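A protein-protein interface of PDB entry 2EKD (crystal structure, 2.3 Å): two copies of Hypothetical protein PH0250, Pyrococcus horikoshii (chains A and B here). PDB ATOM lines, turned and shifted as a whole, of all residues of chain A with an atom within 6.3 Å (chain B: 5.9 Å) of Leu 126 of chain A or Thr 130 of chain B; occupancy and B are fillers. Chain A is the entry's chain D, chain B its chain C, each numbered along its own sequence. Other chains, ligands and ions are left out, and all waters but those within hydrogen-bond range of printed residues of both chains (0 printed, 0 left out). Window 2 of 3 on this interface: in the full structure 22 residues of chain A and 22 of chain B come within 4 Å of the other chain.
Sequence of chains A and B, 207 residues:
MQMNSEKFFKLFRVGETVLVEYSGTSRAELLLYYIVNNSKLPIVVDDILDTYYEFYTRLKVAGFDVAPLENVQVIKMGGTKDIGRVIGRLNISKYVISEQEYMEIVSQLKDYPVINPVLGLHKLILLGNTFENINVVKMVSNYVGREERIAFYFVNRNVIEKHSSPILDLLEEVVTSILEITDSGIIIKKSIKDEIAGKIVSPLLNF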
ATOM      1  N   LEU A 121      20.959  24.819  -8.812  1.00  0.00           N
ATOM      2  CA  LEU A 121      20.439  25.110  -7.474  1.00  0.00           C
ATOM      3  C   LEU A 121      18.922  24.881  -7.359  1.00  0.00           C
ATOM      4  O   LEU A 121      18.449  24.355  -6.349  1.00  0.00           O
ATOM      5  CB  LEU A 121      20.763  26.553  -7.068  1.00  0.00           C
ATOM      6  CG  LEU A 121      20.481  26.918  -5.604  1.00  0.00           C
ATOM      7  CD1 LEU A 121      21.526  26.254  -4.716  1.00  0.00           C
ATOM      8  CD2 LEU A 121      20.533  28.427  -5.412  1.00  0.00           C
ATOM      9  N   HIS A 122      18.162  25.265  -8.385  1.00  0.00           N
ATOM     10  CA  HIS A 122      16.707  25.101  -8.339  1.00  0.00           C
ATOM     11  C   HIS A 122      16.264  23.664  -8.114  1.00  0.00           C
ATOM     12  O   HIS A 122      15.161  23.422  -7.634  1.00  0.00           O
ATOM     13  CB  HIS A 122      16.052  25.632  -9.614  1.00  0.00           C
ATOM     14  CG  HIS A 122      16.659  25.096 -10.868  1.00  0.00           C
ATOM     15  ND1 HIS A 122      17.812  25.616 -11.414  1.00  0.00           N
ATOM     16  CD2 HIS A 122      16.298  24.059 -11.659  1.00  0.00           C
ATOM     17  CE1 HIS A 122      18.138  24.921 -12.490  1.00  0.00           C
ATOM     18  NE2 HIS A 122      17.237  23.971 -12.660  1.00  0.00           N
ATOM     19  N   LYS A 123      17.123  22.711  -8.453  1.00  0.00           N
ATOM     20  CA  LYS A 123      16.792  21.303  -8.260  1.00  0.00           C
ATOM     21  C   LYS A 123      16.758  20.965  -6.773  1.00  0.00           C
ATOM     22  O   LYS A 123      15.869  20.247  -6.312  1.00  0.00           O
ATOM     23  CB  LYS A 123      17.813  20.407  -8.967  1.00  0.00           C
ATOM     24  CG  LYS A 123      17.771  20.502 -10.482  1.00  0.00           C
ATOM     25  CD  LYS A 123      18.734  19.522 -11.129  1.00  0.00           C
ATOM     26  CE  LYS A 123      18.689  19.643 -12.649  1.00  0.00           C
ATOM     27  NZ  LYS A 123      19.576  18.650 -13.311  1.00  0.00           N
ATOM     28  N   LEU A 124      17.733  21.484  -6.034  1.00  0.00           N
ATOM     29  CA  LEU A 124      17.825  21.247  -4.597  1.00  0.00           C
ATOM     30  C   LEU A 124      16.584  21.798  -3.903  1.00  0.00           C
ATOM     31  O   LEU A 124      16.072  21.207  -2.956  1.00  0.00           O
ATOM     32  CB  LEU A 124      19.077  21.927  -4.023  1.00  0.00           C
ATOM     33  CG  LEU A 124      20.432  21.475  -4.573  1.00  0.00           C
ATOM     34  CD1 LEU A 124      21.546  22.310  -3.945  1.00  0.00           C
ATOM     35  CD2 LEU A 124      20.642  19.990  -4.288  1.00  0.00           C
ATOM     36  N   ILE A 125      16.103  22.932  -4.388  1.00  0.00           N
ATOM     37  CA  ILE A 125      14.935  23.567  -3.812  1.00  0.00           C
ATOM     38  C   ILE A 125      13.640  22.825  -4.139  1.00  0.00           C
ATOM     39  O   ILE A 125      12.775  22.668  -3.276  1.00  0.00           O
ATOM     40  CB  ILE A 125      14.850  25.038  -4.285  1.00  0.00           C
ATOM     41  CG1 ILE A 125      16.003  25.834  -3.653  1.00  0.00           C
ATOM     42  CG2 ILE A 125      13.483  25.629  -3.938  1.00  0.00           C
ATOM     43  CD1 ILE A 125      16.123  27.267  -4.131  1.00  0.00           C
ATOM     44  N   LEU A 126      13.507  22.369  -5.379  1.00  0.00           N
ATOM     45  CA  LEU A 126      12.311  21.644  -5.800  1.00  0.00           C
ATOM     46  C   LEU A 126      12.158  20.314  -5.055  1.00  0.00           C
ATOM     47  O   LEU A 126      11.050  19.884  -4.761  1.00  0.00           O
ATOM     48  CB  LEU A 126      12.356  21.373  -7.309  1.00  0.00           C
ATOM     49  CG  LEU A 126      11.149  20.616  -7.871  1.00  0.00           C
ATOM     50  CD1 LEU A 126       9.886  21.426  -7.617  1.00  0.00           C
ATOM     51  CD2 LEU A 126      11.325  20.372  -9.352  1.00  0.00           C
ATOM     52  N   LEU A 127      13.281  19.682  -4.738  1.00  0.00           N
ATOM     53  CA  LEU A 127      13.285  18.390  -4.052  1.00  0.00           C
ATOM     54  C   LEU A 127      13.209  18.421  -2.524  1.00  0.00           C
ATOM     55  O   LEU A 127      12.585  17.551  -1.917  1.00  0.00           O
ATOM     56  CB  LEU A 127      14.533  17.599  -4.457  1.00  0.00           C
ATOM     57  CG  LEU A 127      14.577  17.002  -5.864  1.00  0.00           C
ATOM     58  CD1 LEU A 127      15.998  16.588  -6.215  1.00  0.00           C
ATOM     59  CD2 LEU A 127      13.633  15.807  -5.927  1.00  0.00           C
ATOM     60  N   GLY A 128      13.849  19.406  -1.902  1.00  0.00           N
ATOM     61  CA  GLY A 128      13.850  19.475  -0.449  1.00  0.00           C
ATOM     62  C   GLY A 128      12.573  19.985   0.190  1.00  0.00           C
ATOM     63  O   GLY A 128      11.707  20.535  -0.491  1.00  0.00           O
ATOM     64  N   ASN A 133      14.968  23.858   2.158  1.00  0.00           N
ATOM     65  CA  ASN A 133      15.008  24.971   1.201  1.00  0.00           C
ATOM     66  C   ASN A 133      15.752  26.145   1.864  1.00  0.00           C
ATOM     67  O   ASN A 133      16.618  26.779   1.258  1.00  0.00           O
ATOM     68  CB  ASN A 133      13.582  25.423   0.828  1.00  0.00           C
ATOM     69  CG  ASN A 133      12.874  24.455  -0.118  1.00  0.00           C
ATOM     70  OD1 ASN A 133      11.690  24.626  -0.420  1.00  0.00           O
ATOM     71  ND2 ASN A 133      13.590  23.444  -0.590  1.00  0.00           N
ATOM     72  N   VAL A 159      10.901  27.472 -11.665  1.00  0.00           N
ATOM     73  CA  VAL A 159      10.961  26.269 -10.847  1.00  0.00           C
ATOM     74  C   VAL A 159      10.902  26.656  -9.366  1.00  0.00           C
ATOM     75  O   VAL A 159      10.149  26.060  -8.601  1.00  0.00           O
ATOM     76  CB  VAL A 159      12.262  25.460 -11.121  1.00  0.00           C
ATOM     77  CG1 VAL A 159      12.467  24.410 -10.045  1.00  0.00           C
ATOM     78  CG2 VAL A 159      12.188  24.796 -12.486  1.00  0.00           C
ATOM     79  N   HIS A 163       7.375  26.738  -6.936  1.00  0.00           N
ATOM     80  CA  HIS A 163       7.471  25.692  -5.918  1.00  0.00           C
ATOM     81  C   HIS A 163       7.367  26.325  -4.533  1.00  0.00           C
ATOM     82  O   HIS A 163       6.697  25.791  -3.647  1.00  0.00           O
ATOM     83  CB  HIS A 163       8.787  24.923  -6.008  1.00  0.00           C
ATOM     84  CG  HIS A 163       8.956  23.917  -4.910  1.00  0.00           C
ATOM     85  ND1 HIS A 163       8.182  22.778  -4.818  1.00  0.00           N
ATOM     86  CD2 HIS A 163       9.761  23.915  -3.820  1.00  0.00           C
ATOM     87  CE1 HIS A 163       8.500  22.119  -3.718  1.00  0.00           C
ATOM     88  NE2 HIS A 163       9.455  22.788  -3.095  1.00  0.00           N
ATOM     89  N   GLY B 128       2.563  10.904 -10.994  1.00  0.00           N
ATOM     90  CA  GLY B 128       3.605  10.906  -9.990  1.00  0.00           C
ATOM     91  C   GLY B 128       3.723  12.141  -9.123  1.00  0.00           C
ATOM     92  O   GLY B 128       3.012  13.134  -9.324  1.00  0.00           O
ATOM     93  N   ASN B 129       4.615  12.065  -8.138  1.00  0.00           N
ATOM     94  CA  ASN B 129       4.864  13.189  -7.244  1.00  0.00           C
ATOM     95  C   ASN B 129       6.081  13.926  -7.788  1.00  0.00           C
ATOM     96  O   ASN B 129       6.600  13.577  -8.848  1.00  0.00           O
ATOM     97  CB  ASN B 129       5.128  12.713  -5.802  1.00  0.00           C
ATOM     98  CG  ASN B 129       6.254  11.697  -5.707  1.00  0.00           C
ATOM     99  OD1 ASN B 129       7.247  11.774  -6.431  1.00  0.00           O
ATOM    100  ND2 ASN B 129       6.113  10.748  -4.791  1.00  0.00           N
ATOM    101  N   THR B 130       6.543  14.934  -7.064  1.00  0.00           N
ATOM    102  CA  THR B 130       7.690  15.722  -7.502  1.00  0.00           C
ATOM    103  C   THR B 130       8.963  14.900  -7.724  1.00  0.00           C
ATOM    104  O   THR B 130       9.683  15.111  -8.703  1.00  0.00           O
ATOM    105  CB  THR B 130       7.981  16.839  -6.492  1.00  0.00           C
ATOM    106  OG1 THR B 130       6.817  17.664  -6.362  1.00  0.00           O
ATOM    107  CG2 THR B 130       9.157  17.702  -6.958  1.00  0.00           C
ATOM    108  N   PHE B 131       9.244  13.967  -6.820  1.00  0.00           N
ATOM    109  CA  PHE B 131      10.442  13.143  -6.944  1.00  0.00           C
ATOM    110  C   PHE B 131      10.372  12.282  -8.201  1.00  0.00           C
ATOM    111  O   PHE B 131      11.351  12.146  -8.923  1.00  0.00           O
ATOM    112  CB  PHE B 131      10.602  12.244  -5.711  1.00  0.00           C
ATOM    113  CG  PHE B 131      11.902  11.481  -5.678  1.00  0.00           C
ATOM    114  CD1 PHE B 131      13.109  12.146  -5.471  1.00  0.00           C
ATOM    115  CD2 PHE B 131      11.918  10.101  -5.857  1.00  0.00           C
ATOM    116  CE1 PHE B 131      14.317  11.445  -5.441  1.00  0.00           C
ATOM    117  CE2 PHE B 131      13.114   9.390  -5.828  1.00  0.00           C
ATOM    118  CZ  PHE B 131      14.321  10.063  -5.620  1.00  0.00           C
ATOM    119  N   GLU B 132       9.201  11.714  -8.458  1.00  0.00           N
ATOM    120  CA  GLU B 132       8.996  10.861  -9.627  1.00  0.00           C
ATOM    121  C   GLU B 132       8.990  11.698 -10.905  1.00  0.00           C
ATOM    122  O   GLU B 132       9.533  11.284 -11.931  1.00  0.00           O
ATOM    123  CB  GLU B 132       7.682  10.086  -9.467  1.00  0.00           C
ATOM    124  CG  GLU B 132       7.635   9.313  -8.148  1.00  0.00           C
ATOM    125  CD  GLU B 132       6.266   8.761  -7.798  1.00  0.00           C
ATOM    126  OE1 GLU B 132       5.261   9.491  -7.940  1.00  0.00           O
ATOM    127  OE2 GLU B 132       6.197   7.597  -7.355  1.00  0.00           O
ATOM    128  N   ASN B 133       8.387  12.881 -10.834  1.00  0.00           N
ATOM    129  CA  ASN B 133       8.333  13.773 -11.982  1.00  0.00           C
ATOM    130  C   ASN B 133       9.755  14.147 -12.388  1.00  0.00           C
ATOM    131  O   ASN B 133      10.081  14.184 -13.580  1.00  0.00           O
ATOM    132  CB  ASN B 133       7.553  15.040 -11.640  1.00  0.00           C
ATOM    133  CG  ASN B 133       6.065  14.800 -11.540  1.00  0.00           C
ATOM    134  OD1 ASN B 133       5.318  15.684 -11.128  1.00  0.00           O
ATOM    135  ND2 ASN B 133       5.621  13.611 -11.926  1.00  0.00           N
ATOM    136  N   ILE B 134      10.604  14.420 -11.399  1.00  0.00           N
ATOM    137  CA  ILE B 134      11.985  14.783 -11.689  1.00  0.00           C
ATOM    138  C   ILE B 134      12.710  13.658 -12.420  1.00  0.00           C
ATOM    139  O   ILE B 134      13.519  13.912 -13.315  1.00  0.00           O
ATOM    140  CB  ILE B 134      12.758  15.151 -10.399  1.00  0.00           C
ATOM    141  CG1 ILE B 134      12.322  16.541  -9.935  1.00  0.00           C
ATOM    142  CG2 ILE B 134      14.260  15.099 -10.641  1.00  0.00           C
ATOM    143  CD1 ILE B 134      13.072  17.067  -8.739  1.00  0.00           C
ATOM    144  N   ASN B 135      12.423  12.415 -12.041  1.00  0.00           N
ATOM    145  CA  ASN B 135      13.058  11.284 -12.706  1.00  0.00           C
ATOM    146  C   ASN B 135      12.567  11.189 -14.148  1.00  0.00           C
ATOM    147  O   ASN B 135      13.318  10.802 -15.037  1.00  0.00           O
ATOM    148  CB  ASN B 135      12.785   9.986 -11.947  1.00  0.00           C
ATOM    149  CG  ASN B 135      13.518   9.934 -10.618  1.00  0.00           C
ATOM    150  OD1 ASN B 135      14.675  10.352 -10.522  1.00  0.00           O
ATOM    151  ND2 ASN B 135      12.856   9.413  -9.590  1.00  0.00           N
ATOM    152  N   SER B 164       2.014  20.224 -11.973  1.00  0.00           N
ATOM    153  CA  SER B 164       3.269  20.730 -11.435  1.00  0.00           C
ATOM    154  C   SER B 164       3.877  21.724 -12.419  1.00  0.00           C
ATOM    155  O   SER B 164       4.564  21.337 -13.365  1.00  0.00           O
ATOM    156  CB  SER B 164       4.256  19.584 -11.198  1.00  0.00           C
ATOM    157  OG  SER B 164       5.518  20.086 -10.778  1.00  0.00           O
ATOM    158  N   PRO B 166       6.330  23.711 -11.983  1.00  0.00           N
ATOM    159  CA  PRO B 166       7.797  23.671 -12.008  1.00  0.00           C
ATOM    160  C   PRO B 166       8.308  22.621 -12.985  1.00  0.00           C
ATOM    161  O   PRO B 166       9.300  22.841 -13.688  1.00  0.00           O
ATOM    162  CB  PRO B 166       8.157  23.325 -10.570  1.00  0.00           C
ATOM    163  CG  PRO B 166       7.053  23.969  -9.790  1.00  0.00           C
ATOM    164  CD  PRO B 166       5.835  23.578 -10.602  1.00  0.00           C
ATOM    165  N   ILE B 167       7.621  21.476 -13.014  1.00  0.00           N
ATOM    166  CA  ILE B 167       7.992  20.369 -13.889  1.00  0.00           C
ATOM    167  C   ILE B 167       7.873  20.728 -15.367  1.00  0.00           C
ATOM    168  O   ILE B 167       8.700  20.310 -16.175  1.00  0.00           O
ATOM    169  CB  ILE B 167       7.139  19.116 -13.588  1.00  0.00           C
ATOM    170  CG1 ILE B 167       7.495  18.586 -12.198  1.00  0.00           C
ATOM    171  CG2 ILE B 167       7.376  18.045 -14.645  1.00  0.00           C
ATOM    172  CD1 ILE B 167       8.967  18.205 -12.033  1.00  0.00           C
ATOM    173  N   LEU B 170      10.879  22.707 -16.227  1.00  0.00           N
ATOM    174  CA  LEU B 170      12.106  21.915 -16.279  1.00  0.00           C
ATOM    175  C   LEU B 170      12.160  21.222 -17.638  1.00  0.00           C
ATOM    176  O   LEU B 170      13.197  21.217 -18.301  1.00  0.00           O
ATOM    177  CB  LEU B 170      12.133  20.863 -15.174  1.00  0.00           C
ATOM    178  CG  LEU B 170      12.528  21.329 -13.775  1.00  0.00           C
ATOM    179  CD1 LEU B 170      12.370  20.161 -12.813  1.00  0.00           C
ATOM    180  CD2 LEU B 170      13.974  21.846 -13.771  1.00  0.00           C
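Among the printed residues, pairs that only touch across the chains: His 122 of chain A with Leu 170 of chain B, Leu 126 of chain A with Thr 130 of chain B, Leu 126 of chain A with Ile 134 of chain B, Leu 126 of chain A with Pro 166 of chain B, Leu 126 of chain A with Leu 170 of chain B, Leu 127 of chain A with Phe 131 of chain B, Leu 127 of chain A with Ile 134 of chain B, Val 159 of chain A with Pro 166 of chain B, Val 159 of chain A with Leu 170 of chain B and His 163 of chain A with Pro 166 of chain B.
Of the 12 printed residues of chain B, 5 touch a printed residue of chain A.
Printed residues of chain B that touch a printed residue of chain A: Thr 130, Phe 131, Ile 134, Pro 166 and Leu 170.
Hydrophobic or aromatic side chains of chain B that line the printed part of chain A: Phe 131, Ile 134, Pro 166 and Leu 170.
Along chain B the printed residues that touch a printed residue of chain A span positions 130 to 170.
Among the printed residues, 10 pairs touch across the chains.
Among the printed residues, no Asp or Glu carboxylate lies within 4 Å of a Lys or Arg side-chain nitrogen of the other chain.
Leu 121 of chain A touches none of the printed residues of chain B.
Printed residues of chain B within 4 Å of His 122 of chain A: Leu 170.
Printed residues of chain B within 4 Å of Leu 127 of chain A: Phe 131 (3.7 Å) and Ile 134 (3.1 Å).
Of the printed residues of chain B, His 163 of chain A touches Pro 166.
Printed residues of chain A within 4 Å of Phe 131 of chain B: Leu 127.
Printed residues of chain A within 4 Å of Ile 134 of chain B: Leu 126 (3.8 Å) and Leu 127 (3.1 Å).
The nearest printed residue of chain A that does not touch Pro 166 of chain B is His 122 of chain A (7.4 Å).
The backbone carbonyl oxygen of Phe 131 of chain B sits at hydrogen-bond distance from the side-chain amide nitrogen of Asn 135 of chain B, 3.2 Å away.
NE2 of His 163 of chain A lies close to O of Ile 125 of chain A (3.3 Å).
The side-chain amide oxygen (OD1) of Asn 129 of chain B is in hydrogen-bond range of the backbone NH (N) of Phe 131 of chain B, 3.0 Å away.
Positions printed for both chains: 128 and 133.
Of the 10 pairs that touch across the chains among the printed residues, none has its exchanged pair printed and touching as well.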
